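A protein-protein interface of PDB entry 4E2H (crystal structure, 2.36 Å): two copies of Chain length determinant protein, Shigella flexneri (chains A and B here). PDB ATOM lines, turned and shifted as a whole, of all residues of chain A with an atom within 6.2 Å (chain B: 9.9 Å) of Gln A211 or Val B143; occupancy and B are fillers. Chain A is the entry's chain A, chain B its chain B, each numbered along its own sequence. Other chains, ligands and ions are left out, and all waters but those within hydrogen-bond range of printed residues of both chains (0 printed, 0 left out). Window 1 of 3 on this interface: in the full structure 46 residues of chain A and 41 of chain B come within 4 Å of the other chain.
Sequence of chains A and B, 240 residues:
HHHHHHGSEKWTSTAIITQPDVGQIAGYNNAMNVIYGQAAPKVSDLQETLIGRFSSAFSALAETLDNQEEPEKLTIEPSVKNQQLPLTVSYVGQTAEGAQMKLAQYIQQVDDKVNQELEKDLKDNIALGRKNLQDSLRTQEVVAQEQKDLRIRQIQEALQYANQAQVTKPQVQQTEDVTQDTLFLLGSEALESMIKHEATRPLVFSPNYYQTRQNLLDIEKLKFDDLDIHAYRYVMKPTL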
ATOM      1  N   SER A 206     -21.338  11.018 -17.767  1.00  0.00           N
ATOM      2  CA  SER A 206     -22.609  11.617 -17.340  1.00  0.00           C
ATOM      3  C   SER A 206     -23.135  12.634 -18.339  1.00  0.00           C
ATOM      4  O   SER A 206     -22.337  13.284 -19.043  1.00  0.00           O
ATOM      5  CB  SER A 206     -22.403  12.384 -16.033  1.00  0.00           C
ATOM      6  OG  SER A 206     -22.726  11.589 -14.911  1.00  0.00           O
ATOM      7  N   PRO A 207     -24.478  12.804 -18.385  1.00  0.00           N
ATOM      8  CA  PRO A 207     -25.088  13.956 -19.069  1.00  0.00           C
ATOM      9  C   PRO A 207     -24.523  15.240 -18.474  1.00  0.00           C
ATOM     10  O   PRO A 207     -24.266  16.211 -19.192  1.00  0.00           O
ATOM     11  CB  PRO A 207     -26.582  13.838 -18.712  1.00  0.00           C
ATOM     12  CG  PRO A 207     -26.795  12.379 -18.450  1.00  0.00           C
ATOM     13  CD  PRO A 207     -25.498  11.912 -17.797  1.00  0.00           C
ATOM     14  N   ASN A 208     -24.330  15.225 -17.159  1.00  0.00           N
ATOM     15  CA  ASN A 208     -23.631  16.300 -16.466  1.00  0.00           C
ATOM     16  C   ASN A 208     -22.257  16.613 -17.115  1.00  0.00           C
ATOM     17  O   ASN A 208     -21.889  17.773 -17.289  1.00  0.00           O
ATOM     18  CB  ASN A 208     -23.509  15.929 -14.980  1.00  0.00           C
ATOM     19  CG  ASN A 208     -22.642  16.897 -14.192  1.00  0.00           C
ATOM     20  OD1 ASN A 208     -22.474  18.057 -14.572  1.00  0.00           O
ATOM     21  ND2 ASN A 208     -22.089  16.422 -13.075  1.00  0.00           N
ATOM     22  N   TYR A 209     -21.517  15.580 -17.510  1.00  0.00           N
ATOM     23  CA  TYR A 209     -20.225  15.798 -18.152  1.00  0.00           C
ATOM     24  C   TYR A 209     -20.407  16.600 -19.416  1.00  0.00           C
ATOM     25  O   TYR A 209     -19.704  17.616 -19.645  1.00  0.00           O
ATOM     26  CB  TYR A 209     -19.527  14.487 -18.484  1.00  0.00           C
ATOM     27  CG  TYR A 209     -18.208  14.667 -19.223  1.00  0.00           C
ATOM     28  CD1 TYR A 209     -17.036  14.940 -18.530  1.00  0.00           C
ATOM     29  CD2 TYR A 209     -18.142  14.579 -20.606  1.00  0.00           C
ATOM     30  CE1 TYR A 209     -15.841  15.131 -19.187  1.00  0.00           C
ATOM     31  CE2 TYR A 209     -16.946  14.754 -21.276  1.00  0.00           C
ATOM     32  CZ  TYR A 209     -15.800  15.026 -20.568  1.00  0.00           C
ATOM     33  OH  TYR A 209     -14.600  15.182 -21.237  1.00  0.00           O
ATOM     34  N   TYR A 210     -21.345  16.180 -20.255  1.00  0.00           N
ATOM     35  CA  TYR A 210     -21.450  16.873 -21.529  1.00  0.00           C
ATOM     36  C   TYR A 210     -21.892  18.310 -21.343  1.00  0.00           C
ATOM     37  O   TYR A 210     -21.385  19.201 -22.013  1.00  0.00           O
ATOM     38  CB  TYR A 210     -22.291  16.099 -22.533  1.00  0.00           C
ATOM     39  CG  TYR A 210     -21.632  14.789 -22.896  1.00  0.00           C
ATOM     40  CD1 TYR A 210     -20.467  14.776 -23.641  1.00  0.00           C
ATOM     41  CD2 TYR A 210     -22.158  13.575 -22.478  1.00  0.00           C
ATOM     42  CE1 TYR A 210     -19.835  13.592 -23.976  1.00  0.00           C
ATOM     43  CE2 TYR A 210     -21.535  12.375 -22.802  1.00  0.00           C
ATOM     44  CZ  TYR A 210     -20.374  12.395 -23.556  1.00  0.00           C
ATOM     45  OH  TYR A 210     -19.727  11.237 -23.899  1.00  0.00           O
ATOM     46  N   GLN A 211     -22.799  18.553 -20.410  1.00  0.00           N
ATOM     47  CA  GLN A 211     -23.263  19.933 -20.216  1.00  0.00           C
ATOM     48  C   GLN A 211     -22.204  20.807 -19.551  1.00  0.00           C
ATOM     49  O   GLN A 211     -21.944  21.908 -20.027  1.00  0.00           O
ATOM     50  CB  GLN A 211     -24.562  20.007 -19.440  1.00  0.00           C
ATOM     51  CG  GLN A 211     -24.413  19.656 -17.984  1.00  0.00           C
ATOM     52  CD  GLN A 211     -25.225  20.612 -17.106  1.00  0.00           C
ATOM     53  OE1 GLN A 211     -26.124  21.311 -17.603  1.00  0.00           O
ATOM     54  NE2 GLN A 211     -24.913  20.653 -15.804  1.00  0.00           N
ATOM     55  N   THR A 212     -21.590  20.323 -18.468  1.00  0.00           N
ATOM     56  CA  THR A 212     -20.426  21.003 -17.897  1.00  0.00           C
ATOM     57  C   THR A 212     -19.452  21.353 -18.990  1.00  0.00           C
ATOM     58  O   THR A 212     -18.876  22.437 -18.993  1.00  0.00           O
ATOM     59  CB  THR A 212     -19.629  20.117 -16.949  1.00  0.00           C
ATOM     60  OG1 THR A 212     -20.418  19.799 -15.811  1.00  0.00           O
ATOM     61  CG2 THR A 212     -18.448  20.857 -16.464  1.00  0.00           C
ATOM     62  N   ARG A 213     -19.251  20.438 -19.932  1.00  0.00           N
ATOM     63  CA  ARG A 213     -18.275  20.734 -20.968  1.00  0.00           C
ATOM     64  C   ARG A 213     -18.785  21.857 -21.848  1.00  0.00           C
ATOM     65  O   ARG A 213     -18.031  22.756 -22.246  1.00  0.00           O
ATOM     66  CB  ARG A 213     -17.983  19.520 -21.829  1.00  0.00           C
ATOM     67  CG  ARG A 213     -17.044  19.860 -22.952  1.00  0.00           C
ATOM     68  CD  ARG A 213     -16.487  18.610 -23.629  1.00  0.00           C
ATOM     69  NE  ARG A 213     -17.497  17.989 -24.491  1.00  0.00           N
ATOM     70  CZ  ARG A 213     -17.398  16.767 -25.010  1.00  0.00           C
ATOM     71  NH1 ARG A 213     -16.332  16.014 -24.751  1.00  0.00           N
ATOM     72  NH2 ARG A 213     -18.366  16.310 -25.792  1.00  0.00           N
ATOM     73  N   GLN A 214     -20.076  21.800 -22.152  1.00  0.00           N
ATOM     74  CA  GLN A 214     -20.694  22.836 -22.957  1.00  0.00           C
ATOM     75  C   GLN A 214     -20.777  24.174 -22.209  1.00  0.00           C
ATOM     76  O   GLN A 214     -20.814  25.237 -22.838  1.00  0.00           O
ATOM     77  CB  GLN A 214     -22.085  22.404 -23.432  1.00  0.00           C
ATOM     78  CG  GLN A 214     -22.780  23.424 -24.332  1.00  0.00           C
ATOM     79  CD  GLN A 214     -22.369  23.291 -25.800  1.00  0.00           C
ATOM     80  OE1 GLN A 214     -22.102  22.181 -26.290  1.00  0.00           O
ATOM     81  NE2 GLN A 214     -22.317  24.427 -26.511  1.00  0.00           N
ATOM     82  N   ASN A 215     -20.824  24.141 -20.878  1.00  0.00           N
ATOM     83  CA  ASN A 215     -20.847  25.392 -20.124  1.00  0.00           C
ATOM     84  C   ASN A 215     -19.505  26.042 -20.341  1.00  0.00           C
ATOM     85  O   ASN A 215     -19.396  27.245 -20.601  1.00  0.00           O
ATOM     86  CB  ASN A 215     -21.053  25.145 -18.628  1.00  0.00           C
ATOM     87  CG  ASN A 215     -22.418  24.542 -18.312  1.00  0.00           C
ATOM     88  OD1 ASN A 215     -23.362  24.632 -19.122  1.00  0.00           O
ATOM     89  ND2 ASN A 215     -22.539  23.935 -17.121  1.00  0.00           N
ATOM     90  N   LEU A 216     -18.483  25.205 -20.251  1.00  0.00           N
ATOM     91  CA  LEU A 216     -17.118  25.656 -20.318  1.00  0.00           C
ATOM     92  C   LEU A 216     -16.827  26.280 -21.668  1.00  0.00           C
ATOM     93  O   LEU A 216     -16.120  27.272 -21.755  1.00  0.00           O
ATOM     94  CB  LEU A 216     -16.175  24.493 -20.025  1.00  0.00           C
ATOM     95  CG  LEU A 216     -14.774  24.991 -19.745  1.00  0.00           C
ATOM     96  CD1 LEU A 216     -14.966  26.187 -18.835  1.00  0.00           C
ATOM     97  CD2 LEU A 216     -13.956  23.917 -19.034  1.00  0.00           C
ATOM     98  N   ASP B 135     -30.355  29.751 -25.822  1.00  0.00           N
ATOM     99  CA  ASP B 135     -29.217  29.129 -25.152  1.00  0.00           C
ATOM    100  C   ASP B 135     -29.607  27.795 -24.545  1.00  0.00           C
ATOM    101  O   ASP B 135     -29.163  26.738 -24.988  1.00  0.00           O
ATOM    102  CB  ASP B 135     -28.691  29.999 -24.007  1.00  0.00           C
ATOM    103  CG  ASP B 135     -27.942  31.230 -24.488  1.00  0.00           C
ATOM    104  OD1 ASP B 135     -28.009  31.542 -25.702  1.00  0.00           O
ATOM    105  OD2 ASP B 135     -27.290  31.895 -23.640  1.00  0.00           O
ATOM    106  N   SER B 136     -30.438  27.857 -23.512  1.00  0.00           N
ATOM    107  CA  SER B 136     -30.732  26.687 -22.710  1.00  0.00           C
ATOM    108  C   SER B 136     -31.359  25.579 -23.545  1.00  0.00           C
ATOM    109  O   SER B 136     -31.376  24.420 -23.131  1.00  0.00           O
ATOM    110  CB  SER B 136     -31.640  27.039 -21.543  1.00  0.00           C
ATOM    111  OG  SER B 136     -32.371  25.888 -21.143  1.00  0.00           O
ATOM    112  N   LEU B 137     -31.897  25.927 -24.709  1.00  0.00           N
ATOM    113  CA  LEU B 137     -32.359  24.886 -25.620  1.00  0.00           C
ATOM    114  C   LEU B 137     -31.154  24.281 -26.343  1.00  0.00           C
ATOM    115  O   LEU B 137     -30.843  23.104 -26.188  1.00  0.00           O
ATOM    116  CB  LEU B 137     -33.352  25.430 -26.641  1.00  0.00           C
ATOM    117  CG  LEU B 137     -34.794  25.606 -26.161  1.00  0.00           C
ATOM    118  CD1 LEU B 137     -35.681  25.907 -27.348  1.00  0.00           C
ATOM    119  CD2 LEU B 137     -35.258  24.354 -25.445  1.00  0.00           C
ATOM    120  N   ARG B 138     -30.476  25.103 -27.133  1.00  0.00           N
ATOM    121  CA  ARG B 138     -29.297  24.663 -27.838  1.00  0.00           C
ATOM    122  C   ARG B 138     -28.418  23.800 -26.944  1.00  0.00           C
ATOM    123  O   ARG B 138     -28.008  22.703 -27.335  1.00  0.00           O
ATOM    124  CB  ARG B 138     -28.502  25.856 -28.350  1.00  0.00           C
ATOM    125  CG  ARG B 138     -27.186  25.449 -28.959  1.00  0.00           C
ATOM    126  CD  ARG B 138     -26.444  26.630 -29.554  1.00  0.00           C
ATOM    127  NE  ARG B 138     -26.993  27.910 -29.112  1.00  0.00           N
ATOM    128  CZ  ARG B 138     -26.602  28.575 -28.025  1.00  0.00           C
ATOM    129  NH1 ARG B 138     -25.644  28.082 -27.234  1.00  0.00           N
ATOM    130  NH2 ARG B 138     -27.182  29.732 -27.724  1.00  0.00           N
ATOM    131  N   THR B 139     -28.118  24.291 -25.749  1.00  0.00           N
ATOM    132  CA  THR B 139     -27.282  23.525 -24.826  1.00  0.00           C
ATOM    133  C   THR B 139     -27.844  22.134 -24.536  1.00  0.00           C
ATOM    134  O   THR B 139     -27.098  21.130 -24.516  1.00  0.00           O
ATOM    135  CB  THR B 139     -27.086  24.250 -23.498  1.00  0.00           C
ATOM    136  OG1 THR B 139     -26.157  25.334 -23.683  1.00  0.00           O
ATOM    137  CG2 THR B 139     -26.567  23.266 -22.413  1.00  0.00           C
ATOM    138  N   GLN B 140     -29.153  22.082 -24.306  1.00  0.00           N
ATOM    139  CA  GLN B 140     -29.828  20.837 -23.975  1.00  0.00           C
ATOM    140  C   GLN B 140     -29.972  19.968 -25.220  1.00  0.00           C
ATOM    141  O   GLN B 140     -30.098  18.747 -25.129  1.00  0.00           O
ATOM    142  CB  GLN B 140     -31.193  21.127 -23.368  1.00  0.00           C
ATOM    143  CG  GLN B 140     -31.188  21.071 -21.874  1.00  0.00           C
ATOM    144  CD  GLN B 140     -32.561  21.303 -21.285  1.00  0.00           C
ATOM    145  OE1 GLN B 140     -33.308  22.187 -21.729  1.00  0.00           O
ATOM    146  NE2 GLN B 140     -32.910  20.502 -20.280  1.00  0.00           N
ATOM    147  N   GLU B 141     -29.968  20.607 -26.383  1.00  0.00           N
ATOM    148  CA  GLU B 141     -29.952  19.882 -27.638  1.00  0.00           C
ATOM    149  C   GLU B 141     -28.628  19.131 -27.775  1.00  0.00           C
ATOM    150  O   GLU B 141     -28.591  17.941 -28.091  1.00  0.00           O
ATOM    151  CB  GLU B 141     -30.120  20.850 -28.806  1.00  0.00           C
ATOM    152  CG  GLU B 141     -31.433  20.720 -29.535  1.00  0.00           C
ATOM    153  CD  GLU B 141     -32.269  21.995 -29.476  1.00  0.00           C
ATOM    154  OE1 GLU B 141     -31.672  23.109 -29.571  1.00  0.00           O
ATOM    155  OE2 GLU B 141     -33.520  21.877 -29.327  1.00  0.00           O
ATOM    156  N   VAL B 142     -27.538  19.840 -27.530  1.00  0.00           N
ATOM    157  CA  VAL B 142     -26.201  19.271 -27.669  1.00  0.00           C
ATOM    158  C   VAL B 142     -25.972  18.102 -26.711  1.00  0.00           C
ATOM    159  O   VAL B 142     -25.451  17.054 -27.107  1.00  0.00           O
ATOM    160  CB  VAL B 142     -25.144  20.324 -27.382  1.00  0.00           C
ATOM    161  CG1 VAL B 142     -23.799  19.639 -27.128  1.00  0.00           C
ATOM    162  CG2 VAL B 142     -25.091  21.355 -28.529  1.00  0.00           C
ATOM    163  N   VAL B 143     -26.367  18.293 -25.452  1.00  0.00           N
ATOM    164  CA  VAL B 143     -26.265  17.258 -24.436  1.00  0.00           C
ATOM    165  C   VAL B 143     -26.947  15.965 -24.853  1.00  0.00           C
ATOM    166  O   VAL B 143     -26.409  14.886 -24.603  1.00  0.00           O
ATOM    167  CB  VAL B 143     -26.904  17.705 -23.113  1.00  0.00           C
ATOM    168  CG1 VAL B 143     -27.042  16.534 -22.160  1.00  0.00           C
ATOM    169  CG2 VAL B 143     -26.090  18.824 -22.484  1.00  0.00           C
ATOM    170  N   ALA B 144     -28.137  16.074 -25.460  1.00  0.00           N
ATOM    171  CA  ALA B 144     -28.915  14.891 -25.818  1.00  0.00           C
ATOM    172  C   ALA B 144     -28.418  14.238 -27.104  1.00  0.00           C
ATOM    173  O   ALA B 144     -28.609  13.038 -27.300  1.00  0.00           O
ATOM    174  CB  ALA B 144     -30.373  15.212 -25.932  1.00  0.00           C
ATOM    175  N   GLN B 145     -27.784  15.011 -27.982  1.00  0.00           N
ATOM    176  CA  GLN B 145     -27.254  14.449 -29.224  1.00  0.00           C
ATOM    177  C   GLN B 145     -25.972  13.674 -28.960  1.00  0.00           C
ATOM    178  O   GLN B 145     -25.630  12.722 -29.668  1.00  0.00           O
ATOM    179  CB  GLN B 145     -26.958  15.547 -30.239  1.00  0.00           C
ATOM    180  CG  GLN B 145     -26.388  15.004 -31.535  1.00  0.00           C
ATOM    181  CD  GLN B 145     -27.442  14.292 -32.369  1.00  0.00           C
ATOM    182  OE1 GLN B 145     -28.643  14.535 -32.220  1.00  0.00           O
ATOM    183  NE2 GLN B 145     -26.993  13.420 -33.269  1.00  0.00           N
ATOM    184  N   GLU B 146     -25.244  14.104 -27.942  1.00  0.00           N
ATOM    185  CA  GLU B 146     -24.008  13.428 -27.611  1.00  0.00           C
ATOM    186  C   GLU B 146     -24.304  12.247 -26.711  1.00  0.00           C
ATOM    187  O   GLU B 146     -23.645  11.222 -26.783  1.00  0.00           O
ATOM    188  CB  GLU B 146     -22.999  14.401 -27.017  1.00  0.00           C
ATOM    189  CG  GLU B 146     -22.721  15.532 -28.003  1.00  0.00           C
ATOM    190  CD  GLU B 146     -21.547  16.414 -27.586  1.00  0.00           C
ATOM    191  OE1 GLU B 146     -21.205  16.420 -26.368  1.00  0.00           O
ATOM    192  OE2 GLU B 146     -20.970  17.105 -28.476  1.00  0.00           O
ATOM    193  N   GLN B 147     -25.313  12.379 -25.868  1.00  0.00           N
ATOM    194  CA  GLN B 147     -25.795  11.216 -25.157  1.00  0.00           C
ATOM    195  C   GLN B 147     -26.092  10.118 -26.171  1.00  0.00           C
ATOM    196  O   GLN B 147     -25.639   8.980 -26.031  1.00  0.00           O
ATOM    197  CB  GLN B 147     -27.048  11.555 -24.360  1.00  0.00           C
ATOM    198  CG  GLN B 147     -26.754  12.089 -22.982  1.00  0.00           C
ATOM    199  CD  GLN B 147     -25.929  11.113 -22.152  1.00  0.00           C
ATOM    200  OE1 GLN B 147     -24.697  11.195 -22.111  1.00  0.00           O
ATOM    201  NE2 GLN B 147     -26.608  10.186 -21.480  1.00  0.00           N
ATOM    202  N   LYS B 148     -26.840  10.472 -27.207  1.00  0.00           N
ATOM    203  CA  LYS B 148     -27.222   9.503 -28.222  1.00  0.00           C
ATOM    204  C   LYS B 148     -25.996   8.955 -28.946  1.00  0.00           C
ATOM    205  O   LYS B 148     -25.819   7.740 -29.031  1.00  0.00           O
ATOM    206  CB  LYS B 148     -28.225  10.119 -29.198  1.00  0.00           C
ATOM    207  CG  LYS B 148     -28.566   9.272 -30.402  1.00  0.00           C
ATOM    208  CD  LYS B 148     -29.709   9.921 -31.173  1.00  0.00           C
ATOM    209  CE  LYS B 148     -29.621   9.591 -32.650  1.00  0.00           C
ATOM    210  NZ  LYS B 148     -30.126  10.699 -33.502  1.00  0.00           N
ATOM    211  N   ASP B 149     -25.124   9.833 -29.428  1.00  0.00           N
ATOM    212  CA  ASP B 149     -23.964   9.358 -30.186  1.00  0.00           C
ATOM    213  C   ASP B 149     -23.043   8.422 -29.407  1.00  0.00           C
ATOM    214  O   ASP B 149     -22.545   7.429 -29.952  1.00  0.00           O
ATOM    215  CB  ASP B 149     -23.215  10.516 -30.831  1.00  0.00           C
ATOM    216  CG  ASP B 149     -24.121  11.318 -31.741  1.00  0.00           C
ATOM    217  OD1 ASP B 149     -25.273  10.856 -31.925  1.00  0.00           O
ATOM    218  OD2 ASP B 149     -23.705  12.381 -32.263  1.00  0.00           O
ATOM    219  N   LEU B 150     -22.828   8.719 -28.136  1.00  0.00           N
ATOM    220  CA  LEU B 150     -22.161   7.746 -27.267  1.00  0.00           C
ATOM    221  C   LEU B 150     -22.898   6.401 -27.246  1.00  0.00           C
ATOM    222  O   LEU B 150     -22.273   5.361 -27.342  1.00  0.00           O
ATOM    223  CB  LEU B 150     -22.022   8.265 -25.832  1.00  0.00           C
ATOM    224  CG  LEU B 150     -21.755   7.152 -24.808  1.00  0.00           C
ATOM    225  CD1 LEU B 150     -20.300   6.748 -24.832  1.00  0.00           C
ATOM    226  CD2 LEU B 150     -22.150   7.610 -23.393  1.00  0.00           C
ATOM    227  N   ARG B 151     -24.221   6.415 -27.132  1.00  0.00           N
ATOM    228  CA  ARG B 151     -24.955   5.163 -27.104  1.00  0.00           C
ATOM    229  C   ARG B 151     -24.742   4.457 -28.441  1.00  0.00           C
ATOM    230  O   ARG B 151     -24.538   3.235 -28.461  1.00  0.00           O
ATOM    231  CB  ARG B 151     -26.431   5.366 -26.785  1.00  0.00           C
ATOM    232  CG  ARG B 151     -27.225   4.076 -26.576  1.00  0.00           C
ATOM    233  CD  ARG B 151     -26.441   3.036 -25.732  1.00  0.00           C
ATOM    234  NE  ARG B 151     -27.364   2.059 -25.134  1.00  0.00           N
ATOM    235  CZ  ARG B 151     -27.100   1.293 -24.072  1.00  0.00           C
ATOM    236  NH1 ARG B 151     -25.924   1.362 -23.472  1.00  0.00           N
ATOM    237  NH2 ARG B 151     -28.019   0.449 -23.613  1.00  0.00           N
ATOM    238  N   LEU B 203     -34.270  11.592 -29.827  1.00  0.00           N
ATOM    239  CA  LEU B 203     -33.563  12.183 -28.708  1.00  0.00           C
ATOM    240  C   LEU B 203     -34.417  12.116 -27.452  1.00  0.00           C
ATOM    241  O   LEU B 203     -35.625  12.338 -27.505  1.00  0.00           O
ATOM    242  CB  LEU B 203     -33.219  13.632 -29.022  1.00  0.00           C
ATOM    243  CG  LEU B 203     -32.195  13.730 -30.150  1.00  0.00           C
ATOM    244  CD1 LEU B 203     -31.926  15.185 -30.545  1.00  0.00           C
ATOM    245  CD2 LEU B 203     -30.894  13.009 -29.739  1.00  0.00           C
ATOM    246  N   VAL B 204     -33.801  11.795 -26.323  1.00  0.00           N
ATOM    247  CA  VAL B 204     -34.501  11.873 -25.046  1.00  0.00           C
ATOM    248  C   VAL B 204     -34.154  13.190 -24.327  1.00  0.00           C
ATOM    249  O   VAL B 204     -32.978  13.559 -24.228  1.00  0.00           O
ATOM    250  CB  VAL B 204     -34.185  10.660 -24.167  1.00  0.00           C
ATOM    251  CG1 VAL B 204     -34.343  11.013 -22.713  1.00  0.00           C
ATOM    252  CG2 VAL B 204     -35.107   9.528 -24.520  1.00  0.00           C
ATOM    253  N   PHE B 205     -35.166  13.904 -23.842  1.00  0.00           N
ATOM    254  CA  PHE B 205     -34.928  15.174 -23.151  1.00  0.00           C
ATOM    255  C   PHE B 205     -35.539  15.254 -21.768  1.00  0.00           C
ATOM    256  O   PHE B 205     -36.494  14.546 -21.463  1.00  0.00           O
ATOM    257  CB  PHE B 205     -35.523  16.326 -23.946  1.00  0.00           C
ATOM    258  CG  PHE B 205     -34.881  16.543 -25.269  1.00  0.00           C
ATOM    259  CD1 PHE B 205     -33.634  17.150 -25.354  1.00  0.00           C
ATOM    260  CD2 PHE B 205     -35.529  16.158 -26.440  1.00  0.00           C
ATOM    261  CE1 PHE B 205     -33.036  17.373 -26.583  1.00  0.00           C
ATOM    262  CE2 PHE B 205     -34.933  16.381 -27.683  1.00  0.00           C
ATOM    263  CZ  PHE B 205     -33.683  16.994 -27.754  1.00  0.00           C
ATOM    264  N   SER B 206     -35.021  16.172 -20.959  1.00  0.00           N
ATOM    265  CA  SER B 206     -35.615  16.486 -19.662  1.00  0.00           C
ATOM    266  C   SER B 206     -36.997  17.148 -19.833  1.00  0.00           C
ATOM    267  O   SER B 206     -37.249  17.836 -20.826  1.00  0.00           O
ATOM    268  CB  SER B 206     -34.672  17.410 -18.880  1.00  0.00           C
ATOM    269  OG  SER B 206     -34.847  17.289 -17.478  1.00  0.00           O
ATOM    270  N   ASN B 208     -37.950  19.604 -18.384  1.00  0.00           N
ATOM    271  CA  ASN B 208     -37.600  21.009 -18.473  1.00  0.00           C
ATOM    272  C   ASN B 208     -37.375  21.468 -19.903  1.00  0.00           C
ATOM    273  O   ASN B 208     -37.499  22.656 -20.217  1.00  0.00           O
ATOM    274  CB  ASN B 208     -36.332  21.317 -17.688  1.00  0.00           C
ATOM    275  CG  ASN B 208     -35.791  22.707 -18.002  1.00  0.00           C
ATOM    276  OD1 ASN B 208     -34.902  22.869 -18.850  1.00  0.00           O
ATOM    277  ND2 ASN B 208     -36.355  23.726 -17.338  1.00  0.00           N
ATOM    278  N   TYR B 209     -37.001  20.536 -20.764  1.00  0.00           N
ATOM    279  CA  TYR B 209     -36.765  20.877 -22.145  1.00  0.00           C
ATOM    280  C   TYR B 209     -38.081  21.215 -22.823  1.00  0.00           C
ATOM    281  O   TYR B 209     -38.153  22.179 -23.588  1.00  0.00           O
ATOM    282  CB  TYR B 209     -36.092  19.737 -22.880  1.00  0.00           C
ATOM    283  CG  TYR B 209     -35.968  20.008 -24.349  1.00  0.00           C
ATOM    284  CD1 TYR B 209     -35.017  20.895 -24.835  1.00  0.00           C
ATOM    285  CD2 TYR B 209     -36.809  19.392 -25.253  1.00  0.00           C
ATOM    286  CE1 TYR B 209     -34.905  21.149 -26.201  1.00  0.00           C
ATOM    287  CE2 TYR B 209     -36.704  19.634 -26.615  1.00  0.00           C
ATOM    288  CZ  TYR B 209     -35.755  20.512 -27.087  1.00  0.00           C
ATOM    289  OH  TYR B 209     -35.658  20.746 -28.451  1.00  0.00           O
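The guanidinium group (NH2) of Arg A213 lies within salt-bridge range of the side-chain carboxylate (OE1) of Glu B146 (2.9 Å).
O of Gln A211 sits close to OD1 of Asn A215.
Of chain B, only Val B143 comes within 4 Å of Gln A211.
No residue of chain B comes within 4 Å of Asn A208.
No residue of chain B comes within 4 Å of Thr A212.
Of the printed residues of chain A, Thr B139 touches Gln A214.
Of the printed residues of chain B, Tyr A210 touches Glu B146 (3.3 Å) and Gln B147 (3.4 Å).
The nearest printed residue of chain B that does not touch Tyr A210 is Leu B150 (4.2 Å).
Among the printed residues, pairs that only touch across the chains: Pro A207 with Gln B147 (3.7 Å), Tyr A210 with Glu B146 (3.3 Å), Tyr A210 with Gln B147 (3.4 Å), Gln A211 with Val B143 (3.6 Å), Gln A214 with Thr B139 (3.9 Å) and Gln A214 with Val B142 (3.2 Å).
3 positions are printed for both chains.
Of the 23 printed residues of chain B, 5 touch a printed residue of chain A.
Of the 11 printed residues of chain A, 5 touch a printed residue of chain B.
Hydrophobic or aromatic side chains of chain A that line the printed part of chain B: Pro A207 and Tyr A210.
Among the printed residues, 7 pairs touch across the chains.
Among the printed residues, Asp or Glu carboxylates within 4 Å of a Lys or Arg side-chain nitrogen of the other chain: Arg A213 with Glu B146 (2.9 Å).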
